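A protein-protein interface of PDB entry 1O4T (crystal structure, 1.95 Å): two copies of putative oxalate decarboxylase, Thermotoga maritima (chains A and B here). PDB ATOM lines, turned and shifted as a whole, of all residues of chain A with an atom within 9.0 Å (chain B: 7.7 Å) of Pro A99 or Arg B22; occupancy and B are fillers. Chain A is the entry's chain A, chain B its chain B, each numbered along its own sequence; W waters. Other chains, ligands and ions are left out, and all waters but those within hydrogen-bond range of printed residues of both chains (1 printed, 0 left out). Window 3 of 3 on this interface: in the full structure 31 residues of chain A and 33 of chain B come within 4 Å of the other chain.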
ATOM      1  N   TYR A  83      -0.224  -9.803  21.623  1.00  0.00           N
ATOM      2  CA  TYR A  83       0.933 -10.025  20.755  1.00  0.00           C
ATOM      3  C   TYR A  83       1.041  -8.858  19.747  1.00  0.00           C
ATOM      4  O   TYR A  83       0.154  -8.615  18.907  1.00  0.00           O
ATOM      5  CB  TYR A  83       0.856 -11.383  20.053  1.00  0.00           C
ATOM      6  CG  TYR A  83       2.110 -11.659  19.253  1.00  0.00           C
ATOM      7  CD1 TYR A  83       3.162 -12.370  19.805  1.00  0.00           C
ATOM      8  CD2 TYR A  83       2.249 -11.189  17.972  1.00  0.00           C
ATOM      9  CE1 TYR A  83       4.365 -12.577  19.099  1.00  0.00           C
ATOM     10  CE2 TYR A  83       3.433 -11.403  17.231  1.00  0.00           C
ATOM     11  CZ  TYR A  83       4.495 -12.115  17.812  1.00  0.00           C
ATOM     12  OH  TYR A  83       5.668 -12.322  17.118  1.00  0.00           O
ATOM     13  N   ILE A  84       2.129  -8.109  19.847  1.00  0.00           N
ATOM     14  CA  ILE A  84       2.306  -6.928  19.012  1.00  0.00           C
ATOM     15  C   ILE A  84       2.701  -7.348  17.604  1.00  0.00           C
ATOM     16  O   ILE A  84       3.747  -7.990  17.404  1.00  0.00           O
ATOM     17  CB  ILE A  84       3.377  -5.975  19.609  1.00  0.00           C
ATOM     18  CG1 ILE A  84       3.147  -5.702  21.099  1.00  0.00           C
ATOM     19  CG2 ILE A  84       3.450  -4.646  18.802  1.00  0.00           C
ATOM     20  CD1 ILE A  84       1.722  -5.220  21.441  1.00  0.00           C
ATOM     21  N   GLY A  87       4.256  -1.899  14.395  1.00  0.00           N
ATOM     22  CA  GLY A  87       4.413  -0.581  14.987  1.00  0.00           C
ATOM     23  C   GLY A  87       5.076  -0.593  16.352  1.00  0.00           C
ATOM     24  O   GLY A  87       5.680  -1.581  16.779  1.00  0.00           O
ATOM     25  N   GLU A  88       4.908   0.515  17.054  1.00  0.00           N
ATOM     26  CA  GLU A  88       5.551   0.767  18.324  1.00  0.00           C
ATOM     27  C   GLU A  88       4.589   1.466  19.290  1.00  0.00           C
ATOM     28  O   GLU A  88       3.646   2.120  18.893  1.00  0.00           O
ATOM     29  CB  GLU A  88       6.747   1.713  18.094  1.00  0.00           C
ATOM     30  CG  GLU A  88       8.006   1.012  17.677  1.00  0.00           C
ATOM     31  CD  GLU A  88       9.090   1.997  17.230  1.00  0.00           C
ATOM     32  OE1 GLU A  88      10.115   1.519  16.681  1.00  0.00           O
ATOM     33  OE2 GLU A  88       8.892   3.225  17.418  1.00  0.00           O
ATOM     34  N   GLY A  89       4.870   1.353  20.568  1.00  0.00           N
ATOM     35  CA  GLY A  89       4.073   2.022  21.564  1.00  0.00           C
ATOM     36  C   GLY A  89       4.528   1.747  22.982  1.00  0.00           C
ATOM     37  O   GLY A  89       5.654   1.327  23.216  1.00  0.00           O
ATOM     38  N   VAL A  90       3.645   2.038  23.931  1.00  0.00           N
ATOM     39  CA  VAL A  90       3.949   1.883  25.340  1.00  0.00           C
ATOM     40  C   VAL A  90       2.804   1.106  26.003  1.00  0.00           C
ATOM     41  O   VAL A  90       1.631   1.469  25.876  1.00  0.00           O
ATOM     42  CB  VAL A  90       4.128   3.224  26.025  1.00  0.00           C
ATOM     43  CG1 VAL A  90       4.486   3.001  27.445  1.00  0.00           C
ATOM     44  CG2 VAL A  90       5.200   4.044  25.361  1.00  0.00           C
ATOM     45  N   PHE A  91       3.166  -0.003  26.641  1.00  0.00           N
ATOM     46  CA  PHE A  91       2.283  -0.846  27.409  1.00  0.00           C
ATOM     47  C   PHE A  91       2.402  -0.497  28.887  1.00  0.00           C
ATOM     48  O   PHE A  91       3.513  -0.401  29.433  1.00  0.00           O
ATOM     49  CB  PHE A  91       2.722  -2.288  27.192  1.00  0.00           C
ATOM     50  CG  PHE A  91       1.921  -3.286  27.952  1.00  0.00           C
ATOM     51  CD1 PHE A  91       0.572  -3.464  27.681  1.00  0.00           C
ATOM     52  CD2 PHE A  91       2.507  -4.085  28.902  1.00  0.00           C
ATOM     53  CE1 PHE A  91      -0.188  -4.407  28.353  1.00  0.00           C
ATOM     54  CE2 PHE A  91       1.724  -5.057  29.594  1.00  0.00           C
ATOM     55  CZ  PHE A  91       0.381  -5.189  29.309  1.00  0.00           C
ATOM     56  N   HIS A  92       1.276  -0.236  29.523  1.00  0.00           N
ATOM     57  CA  HIS A  92       1.245   0.028  30.941  1.00  0.00           C
ATOM     58  C   HIS A  92       0.682  -1.196  31.641  1.00  0.00           C
ATOM     59  O   HIS A  92      -0.419  -1.629  31.317  1.00  0.00           O
ATOM     60  CB  HIS A  92       0.350   1.237  31.260  1.00  0.00           C
ATOM     61  CG  HIS A  92       0.327   1.617  32.714  1.00  0.00           C
ATOM     62  ND1 HIS A  92       1.146   2.595  33.243  1.00  0.00           N
ATOM     63  CD2 HIS A  92      -0.411   1.151  33.754  1.00  0.00           C
ATOM     64  CE1 HIS A  92       0.920   2.711  34.539  1.00  0.00           C
ATOM     65  NE2 HIS A  92      -0.028   1.856  34.875  1.00  0.00           N
ATOM     66  N   LYS A  96       3.621   0.345  35.684  1.00  0.00           N
ATOM     67  CA  LYS A  96       4.857   0.625  34.929  1.00  0.00           C
ATOM     68  C   LYS A  96       4.581   0.821  33.437  1.00  0.00           C
ATOM     69  O   LYS A  96       3.784   0.112  32.871  1.00  0.00           O
ATOM     70  CB  LYS A  96       5.869  -0.527  35.103  1.00  0.00           C
ATOM     71  N   ASP A  97       5.250   1.788  32.814  1.00  0.00           N
ATOM     72  CA  ASP A  97       5.288   1.875  31.344  1.00  0.00           C
ATOM     73  C   ASP A  97       6.497   1.179  30.758  1.00  0.00           C
ATOM     74  O   ASP A  97       7.619   1.432  31.184  1.00  0.00           O
ATOM     75  CB  ASP A  97       5.331   3.321  30.886  1.00  0.00           C
ATOM     76  CG  ASP A  97       4.115   4.091  31.317  1.00  0.00           C
ATOM     77  OD1 ASP A  97       2.996   3.556  31.318  1.00  0.00           O
ATOM     78  OD2 ASP A  97       4.195   5.259  31.677  1.00  0.00           O
ATOM     79  N   VAL A  98       6.248   0.365  29.742  1.00  0.00           N
ATOM     80  CA  VAL A  98       7.266  -0.401  29.039  1.00  0.00           C
ATOM     81  C   VAL A  98       7.078  -0.155  27.532  1.00  0.00           C
ATOM     82  O   VAL A  98       5.987  -0.378  27.018  1.00  0.00           O
ATOM     83  CB  VAL A  98       7.074  -1.902  29.359  1.00  0.00           C
ATOM     84  CG1 VAL A  98       7.896  -2.791  28.439  1.00  0.00           C
ATOM     85  CG2 VAL A  98       7.412  -2.180  30.838  1.00  0.00           C
ATOM     86  N   PRO A  99       8.099   0.327  26.823  1.00  0.00           N
ATOM     87  CA  PRO A  99       7.995   0.440  25.378  1.00  0.00           C
ATOM     88  C   PRO A  99       7.972  -0.913  24.698  1.00  0.00           C
ATOM     89  O   PRO A  99       8.740  -1.806  25.064  1.00  0.00           O
ATOM     90  CB  PRO A  99       9.235   1.228  24.948  1.00  0.00           C
ATOM     91  CG  PRO A  99      10.098   1.402  26.153  1.00  0.00           C
ATOM     92  CD  PRO A  99       9.375   0.835  27.345  1.00  0.00           C
ATOM     93  N   ILE A 100       7.079  -1.033  23.710  1.00  0.00           N
ATOM     94  CA  ILE A 100       6.850  -2.264  23.007  1.00  0.00           C
ATOM     95  C   ILE A 100       6.922  -2.052  21.503  1.00  0.00           C
ATOM     96  O   ILE A 100       6.856  -0.906  20.996  1.00  0.00           O
ATOM     97  CB  ILE A 100       5.539  -2.963  23.448  1.00  0.00           C
ATOM     98  CG1 ILE A 100       4.314  -2.044  23.500  1.00  0.00           C
ATOM     99  CG2 ILE A 100       5.723  -3.558  24.834  1.00  0.00           C
ATOM    100  CD1 ILE A 100       3.691  -1.759  22.183  1.00  0.00           C
ATOM    101  N   LYS A 101       7.127  -3.179  20.825  1.00  0.00           N
ATOM    102  CA  LYS A 101       7.233  -3.247  19.392  1.00  0.00           C
ATOM    103  C   LYS A 101       6.816  -4.634  18.910  1.00  0.00           C
ATOM    104  O   LYS A 101       6.674  -5.589  19.703  1.00  0.00           O
ATOM    105  CB  LYS A 101       8.662  -2.946  18.953  1.00  0.00           C
ATOM    106  CG  LYS A 101       9.693  -3.880  19.545  1.00  0.00           C
ATOM    107  CD  LYS A 101      11.075  -3.501  19.078  1.00  0.00           C
ATOM    108  CE  LYS A 101      11.988  -4.717  19.058  1.00  0.00           C
ATOM    109  NZ  LYS A 101      13.362  -4.270  18.712  1.00  0.00           N
ATOM    110  N   ALA A 102       6.649  -4.717  17.588  1.00  0.00           N
ATOM    111  CA  ALA A 102       6.394  -5.963  16.900  1.00  0.00           C
ATOM    112  C   ALA A 102       7.199  -7.110  17.482  1.00  0.00           C
ATOM    113  O   ALA A 102       8.413  -7.026  17.660  1.00  0.00           O
ATOM    114  CB  ALA A 102       6.692  -5.797  15.413  1.00  0.00           C
ATOM    115  N   GLY A 103       6.503  -8.192  17.785  1.00  0.00           N
ATOM    116  CA  GLY A 103       7.146  -9.377  18.336  1.00  0.00           C
ATOM    117  C   GLY A 103       7.014  -9.492  19.852  1.00  0.00           C
ATOM    118  O   GLY A 103       7.267 -10.542  20.414  1.00  0.00           O
ATOM    119  N   ASP A 104       6.623  -8.408  20.520  1.00  0.00           N
ATOM    120  CA  ASP A 104       6.473  -8.433  21.983  1.00  0.00           C
ATOM    121  C   ASP A 104       5.163  -9.070  22.431  1.00  0.00           C
ATOM    122  O   ASP A 104       4.087  -8.855  21.853  1.00  0.00           O
ATOM    123  CB  ASP A 104       6.576  -7.023  22.555  1.00  0.00           C
ATOM    124  CG  ASP A 104       7.976  -6.443  22.465  1.00  0.00           C
ATOM    125  OD1 ASP A 104       8.994  -7.148  22.197  1.00  0.00           O
ATOM    126  OD2 ASP A 104       8.148  -5.233  22.637  1.00  0.00           O
ATOM    127  N   VAL A 105       5.248  -9.833  23.501  1.00  0.00           N
ATOM    128  CA  VAL A 105       4.057 -10.372  24.172  1.00  0.00           C
ATOM    129  C   VAL A 105       3.833  -9.529  25.416  1.00  0.00           C
ATOM    130  O   VAL A 105       4.760  -9.343  26.192  1.00  0.00           O
ATOM    131  CB  VAL A 105       4.277 -11.819  24.587  1.00  0.00           C
ATOM    132  CG1 VAL A 105       3.116 -12.358  25.433  1.00  0.00           C
ATOM    133  CG2 VAL A 105       4.501 -12.678  23.369  1.00  0.00           C
ATOM    134  N   CYS A 106       2.603  -9.030  25.599  1.00  0.00           N
ATOM    135  CA  CYS A 106       2.218  -8.318  26.834  1.00  0.00           C
ATOM    136  C   CYS A 106       1.208  -9.145  27.568  1.00  0.00           C
ATOM    137  O   CYS A 106       0.152  -9.445  27.003  1.00  0.00           O
ATOM    138  CB  CYS A 106       1.620  -6.959  26.502  1.00  0.00           C
ATOM    139  SG  CYS A 106       2.620  -5.979  25.380  1.00  0.00           S
ATOM    140  N   ILE A 116      -2.642   0.685  26.695  1.00  0.00           N
ATOM    141  CA  ILE A 116      -1.613   0.655  25.669  1.00  0.00           C
ATOM    142  C   ILE A 116      -1.786   1.853  24.767  1.00  0.00           C
ATOM    143  O   ILE A 116      -2.921   2.187  24.385  1.00  0.00           O
ATOM    144  CB  ILE A 116      -1.660  -0.705  24.873  1.00  0.00           C
ATOM    145  CG1 ILE A 116      -0.559  -0.785  23.817  1.00  0.00           C
ATOM    146  CG2 ILE A 116      -3.010  -0.938  24.229  1.00  0.00           C
ATOM    147  CD1 ILE A 116      -0.248  -2.250  23.350  1.00  0.00           C
ATOM    148  N   GLU A 117      -0.677   2.517  24.463  1.00  0.00           N
ATOM    149  CA  GLU A 117      -0.694   3.718  23.636  1.00  0.00           C
ATOM    150  C   GLU A 117       0.244   3.621  22.434  1.00  0.00           C
ATOM    151  O   GLU A 117       1.406   3.170  22.551  1.00  0.00           O
ATOM    152  CB  GLU A 117      -0.312   4.940  24.474  1.00  0.00           C
ATOM    153  CG  GLU A 117      -0.557   6.243  23.737  1.00  0.00           C
ATOM    154  CD  GLU A 117      -0.340   7.490  24.584  1.00  0.00           C
ATOM    155  OE1 GLU A 117      -0.438   7.407  25.826  1.00  0.00           O
ATOM    156  OE2 GLU A 117      -0.103   8.561  23.985  1.00  0.00           O
ATOM    157  N   THR A 119       2.669   5.467  20.444  1.00  0.00           N
ATOM    158  CA  THR A 119       3.534   6.631  20.516  1.00  0.00           C
ATOM    159  C   THR A 119       4.346   6.815  19.210  1.00  0.00           C
ATOM    160  O   THR A 119       5.251   7.617  19.167  1.00  0.00           O
ATOM    161  CB  THR A 119       4.467   6.506  21.741  1.00  0.00           C
ATOM    162  OG1 THR A 119       5.160   5.265  21.694  1.00  0.00           O
ATOM    163  CG2 THR A 119       3.673   6.363  23.034  1.00  0.00           C
ATOM    164  N   LEU A 124      -0.122   1.035  15.192  1.00  0.00           N
ATOM    165  CA  LEU A 124       0.262  -0.033  16.095  1.00  0.00           C
ATOM    166  C   LEU A 124      -0.842  -1.109  16.005  1.00  0.00           C
ATOM    167  O   LEU A 124      -1.982  -0.822  16.307  1.00  0.00           O
ATOM    168  CB  LEU A 124       0.350   0.493  17.527  1.00  0.00           C
ATOM    169  CG  LEU A 124       0.470  -0.461  18.714  1.00  0.00           C
ATOM    170  CD1 LEU A 124       1.770  -1.249  18.685  1.00  0.00           C
ATOM    171  CD2 LEU A 124       0.354   0.376  19.977  1.00  0.00           C
ATOM    172  N   MET B  19       4.027  -8.556  32.727  1.00  0.00           N
ATOM    173  CA  MET B  19       5.344  -8.812  32.094  1.00  0.00           C
ATOM    174  C   MET B  19       5.251  -8.637  30.579  1.00  0.00           C
ATOM    175  O   MET B  19       4.183  -8.788  29.963  1.00  0.00           O
ATOM    176  CB  MET B  19       5.862 -10.221  32.420  1.00  0.00           C
ATOM    177  CG  MET B  19       5.000 -11.386  31.861  1.00  0.00           C
ATOM    178  SD  MET B  19       5.710 -13.105  32.093  1.00  0.00           S
ATOM    179  CE  MET B  19       6.464 -12.966  33.843  1.00  0.00           C
ATOM    180  N   VAL B  20       6.387  -8.280  30.004  1.00  0.00           N
ATOM    181  CA  VAL B  20       6.547  -8.212  28.581  1.00  0.00           C
ATOM    182  C   VAL B  20       7.623  -9.212  28.250  1.00  0.00           C
ATOM    183  O   VAL B  20       8.621  -9.282  28.932  1.00  0.00           O
ATOM    184  CB  VAL B  20       6.928  -6.804  28.138  1.00  0.00           C
ATOM    185  CG1 VAL B  20       7.351  -6.783  26.660  1.00  0.00           C
ATOM    186  CG2 VAL B  20       5.734  -5.841  28.412  1.00  0.00           C
ATOM    187  N   VAL B  21       7.365 -10.008  27.217  1.00  0.00           N
ATOM    188  CA  VAL B  21       8.296 -10.993  26.686  1.00  0.00           C
ATOM    189  C   VAL B  21       8.617 -10.572  25.250  1.00  0.00           C
ATOM    190  O   VAL B  21       7.716 -10.438  24.420  1.00  0.00           O
ATOM    191  CB  VAL B  21       7.617 -12.398  26.686  1.00  0.00           C
ATOM    192  CG1 VAL B  21       8.494 -13.446  25.989  1.00  0.00           C
ATOM    193  CG2 VAL B  21       7.279 -12.833  28.123  1.00  0.00           C
ATOM    194  N   ARG B  22       9.887 -10.359  24.957  1.00  0.00           N
ATOM    195  CA  ARG B  22      10.319  -9.932  23.631  1.00  0.00           C
ATOM    196  C   ARG B  22      10.730 -11.142  22.783  1.00  0.00           C
ATOM    197  O   ARG B  22      11.777 -11.739  22.992  1.00  0.00           O
ATOM    198  CB  ARG B  22      11.453  -8.908  23.757  1.00  0.00           C
ATOM    199  CG  ARG B  22      12.062  -8.463  22.406  1.00  0.00           C
ATOM    200  CD  ARG B  22      12.659  -7.021  22.390  1.00  0.00           C
ATOM    201  NE  ARG B  22      11.601  -6.027  22.647  1.00  0.00           N
ATOM    202  CZ  ARG B  22      11.782  -4.718  22.833  1.00  0.00           C
ATOM    203  NH1 ARG B  22      13.002  -4.172  22.795  1.00  0.00           N
ATOM    204  NH2 ARG B  22      10.722  -3.946  23.063  1.00  0.00           N
ATOM    205  N   SER B  23       9.871 -11.508  21.838  1.00  0.00           N
ATOM    206  CA  SER B  23      10.058 -12.696  20.970  1.00  0.00           C
ATOM    207  C   SER B  23      11.450 -12.900  20.474  1.00  0.00           C
ATOM    208  O   SER B  23      11.948 -14.038  20.448  1.00  0.00           O
ATOM    209  CB  SER B  23       9.249 -12.555  19.686  1.00  0.00           C
ATOM    210  OG  SER B  23       8.003 -13.105  19.850  1.00  0.00           O
ATOM    211  N   SER B  24      12.042 -11.799  19.998  1.00  0.00           N
ATOM    212  CA  SER B  24      13.340 -11.855  19.338  1.00  0.00           C
ATOM    213  C   SER B  24      14.410 -12.321  20.318  1.00  0.00           C
ATOM    214  O   SER B  24      15.463 -12.793  19.901  1.00  0.00           O
ATOM    215  CB  SER B  24      13.709 -10.498  18.713  1.00  0.00           C
ATOM    216  OG  SER B  24      13.954  -9.502  19.704  1.00  0.00           O
ATOM    217  N   GLU B  25      14.156 -12.186  21.613  1.00  0.00           N
ATOM    218  CA  GLU B  25      15.142 -12.514  22.601  1.00  0.00           C
ATOM    219  C   GLU B  25      14.972 -13.922  23.161  1.00  0.00           C
ATOM    220  O   GLU B  25      15.708 -14.316  24.049  1.00  0.00           O
ATOM    221  CB  GLU B  25      15.067 -11.497  23.717  1.00  0.00           C
ATOM    222  CG  GLU B  25      15.434 -10.090  23.244  1.00  0.00           C
ATOM    223  CD  GLU B  25      15.384  -9.051  24.362  1.00  0.00           C
ATOM    224  OE1 GLU B  25      14.967  -9.388  25.506  1.00  0.00           O
ATOM    225  OE2 GLU B  25      15.773  -7.884  24.090  1.00  0.00           O
ATOM    226  N   ILE B  26      14.005 -14.685  22.654  1.00  0.00           N
ATOM    227  CA  ILE B  26      13.808 -16.062  23.118  1.00  0.00           C
ATOM    228  C   ILE B  26      14.590 -16.949  22.167  1.00  0.00           C
ATOM    229  O   ILE B  26      14.504 -16.782  20.945  1.00  0.00           O
ATOM    230  CB  ILE B  26      12.280 -16.420  23.165  1.00  0.00           C
ATOM    231  CG1 ILE B  26      11.613 -15.634  24.301  1.00  0.00           C
ATOM    232  CG2 ILE B  26      12.085 -17.907  23.374  1.00  0.00           C
ATOM    233  CD1 ILE B  26      10.129 -15.641  24.245  1.00  0.00           C
ATOM    234  N   THR B  27      15.368 -17.875  22.701  1.00  0.00           N
ATOM    235  CA  THR B  27      16.052 -18.854  21.841  1.00  0.00           C
ATOM    236  C   THR B  27      15.039 -19.942  21.437  1.00  0.00           C
ATOM    237  O   THR B  27      14.452 -20.611  22.299  1.00  0.00           O
ATOM    238  CB  THR B  27      17.315 -19.441  22.554  1.00  0.00           C
ATOM    239  OG1 THR B  27      18.225 -18.378  22.873  1.00  0.00           O
ATOM    240  CG2 THR B  27      18.130 -20.384  21.610  1.00  0.00           C
ATOM    241  N   LEU B  46       6.464 -18.820  24.278  1.00  0.00           N
ATOM    242  CA  LEU B  46       6.342 -17.425  24.678  1.00  0.00           C
ATOM    243  C   LEU B  46       5.790 -17.278  26.069  1.00  0.00           C
ATOM    244  O   LEU B  46       6.180 -16.363  26.767  1.00  0.00           O
ATOM    245  CB  LEU B  46       5.462 -16.653  23.692  1.00  0.00           C
ATOM    246  CG  LEU B  46       5.976 -16.631  22.260  1.00  0.00           C
ATOM    247  CD1 LEU B  46       4.926 -15.914  21.412  1.00  0.00           C
ATOM    248  CD2 LEU B  46       7.352 -16.044  22.043  1.00  0.00           C
ATOM    249  N   ARG B  61       5.554 -19.139  19.041  1.00  0.00           N
ATOM    250  CA  ARG B  61       5.802 -18.582  17.723  1.00  0.00           C
ATOM    251  C   ARG B  61       6.640 -19.602  16.923  1.00  0.00           C
ATOM    252  O   ARG B  61       7.771 -19.960  17.303  1.00  0.00           O
ATOM    253  CB  ARG B  61       6.557 -17.269  17.838  1.00  0.00           C
ATOM    254  CG  ARG B  61       6.837 -16.556  16.520  1.00  0.00           C
ATOM    255  CD  ARG B  61       7.608 -15.274  16.729  1.00  0.00           C
ATOM    256  NE  ARG B  61       8.016 -14.632  15.482  1.00  0.00           N
ATOM    257  CZ  ARG B  61       8.677 -13.475  15.394  1.00  0.00           C
ATOM    258  NH1 ARG B  61       8.987 -12.783  16.503  1.00  0.00           N
ATOM    259  NH2 ARG B  61       9.043 -13.000  14.193  1.00  0.00           N
HETATM  260  O   HOH W   1      14.943  -6.304  19.545  1.00  0.00           O
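Hydrophobic or aromatic side chains of chain A that line the printed part of chain B: Tyr A83, Phe A91, Val A98 and Val A105.
Along chain B the printed residues that touch a printed residue of chain A span positions 19 to 61.
Among the printed residues, Asp or Glu carboxylates within 4 Å of a Lys or Arg side-chain nitrogen of the other chain: Asp A104 with Arg B22 (2.9 Å).
No position is printed for both chains.
Of the 14 pairs that touch across the chains among the printed residues, none has its exchanged pair printed and touching as well.
The side-chain hydroxyl of Tyr A83 lies within hydrogen-bond range of the guanidinium group of Arg B61 (3.4 Å).
O of Gly A103 is in hydrogen-bond range of OG of Ser B23, at 2.7 Å.
The side-chain carboxylate (OD1) of Asp A104 lies within salt-bridge range of the guanidinium group (NE) of Arg B22, 2.9 Å away.
N of Val A105 lies within hydrogen-bond range of O of Val B21 (2.7 Å).
OG of Ser B23 touches OH of Tyr A83 (3.7 Å).
CG2 of Val B20 touches CD2 of Phe A91, 3.7 Å away.
CG1 of Val A98 touches CG2 of Val B20 (3.7 Å).
Arg B22 touches Pro A99.
Arg B22 touches Lys A101 (NH2 to CG, 3.7 Å).
Asp A104 touches Val B21.
O of Val A105 touches O of Met B19, at 3.9 Å.
CA of Val B20 touches O of Val A105, 3.2 Å away.
CG2 of Val A105 touches CD1 of Leu B46, 3.8 Å away.
O of Met B19 touches CA of Cys A106, at 3.7 Å.
Pro A99 touches one residue of chain B.
Of the printed residues of chain A, Arg B22 touches Pro A99 (3.5 Å), Lys A101 (3.7 Å) and Asp A104 (2.9 Å).
Val B21 touches two residues of chain A.
Ser B23 touches just these residues of chain A: Tyr A83 (3.7 Å) and Gly A103 (2.7 Å).
No residue of chain A comes within 4 Å of Ser B24.
Printed residues of chain A within 4 Å of Val B20: Phe A91, Val A98 and Val A105.
Of the printed residues of chain B, Phe A91 touches Val B20 (3.7 Å).
Of the printed residues of chain A, Met B19 touches Val A105 and Cys A106.
Of the printed residues of chain A, Arg B61 touches Tyr A83 (3.4 Å).
The nearest residue of chain B that does not touch Pro A99 is Val B20 (5.4 Å).
Water W1 bridges the side-chain amino group of Lys A101 (2.7 Å) and the side-chain hydroxyl of Ser B24 (3.4 Å).
The backbone carbonyl oxygen (O) of Ile A84 is in hydrogen-bond range of the backbone NH (N) of Gly A103 (2.8 Å).
The backbone NH (N) of Ile A84 sits at hydrogen-bond distance from the backbone carbonyl oxygen (O) of Asp A104, 2.9 Å away.
The backbone carbonyl oxygen of Phe A91 lies within hydrogen-bond range of the backbone NH of Val A98.
N of Lys A101 sits at hydrogen-bond distance from OD2 of Asp A104 (2.9 Å).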
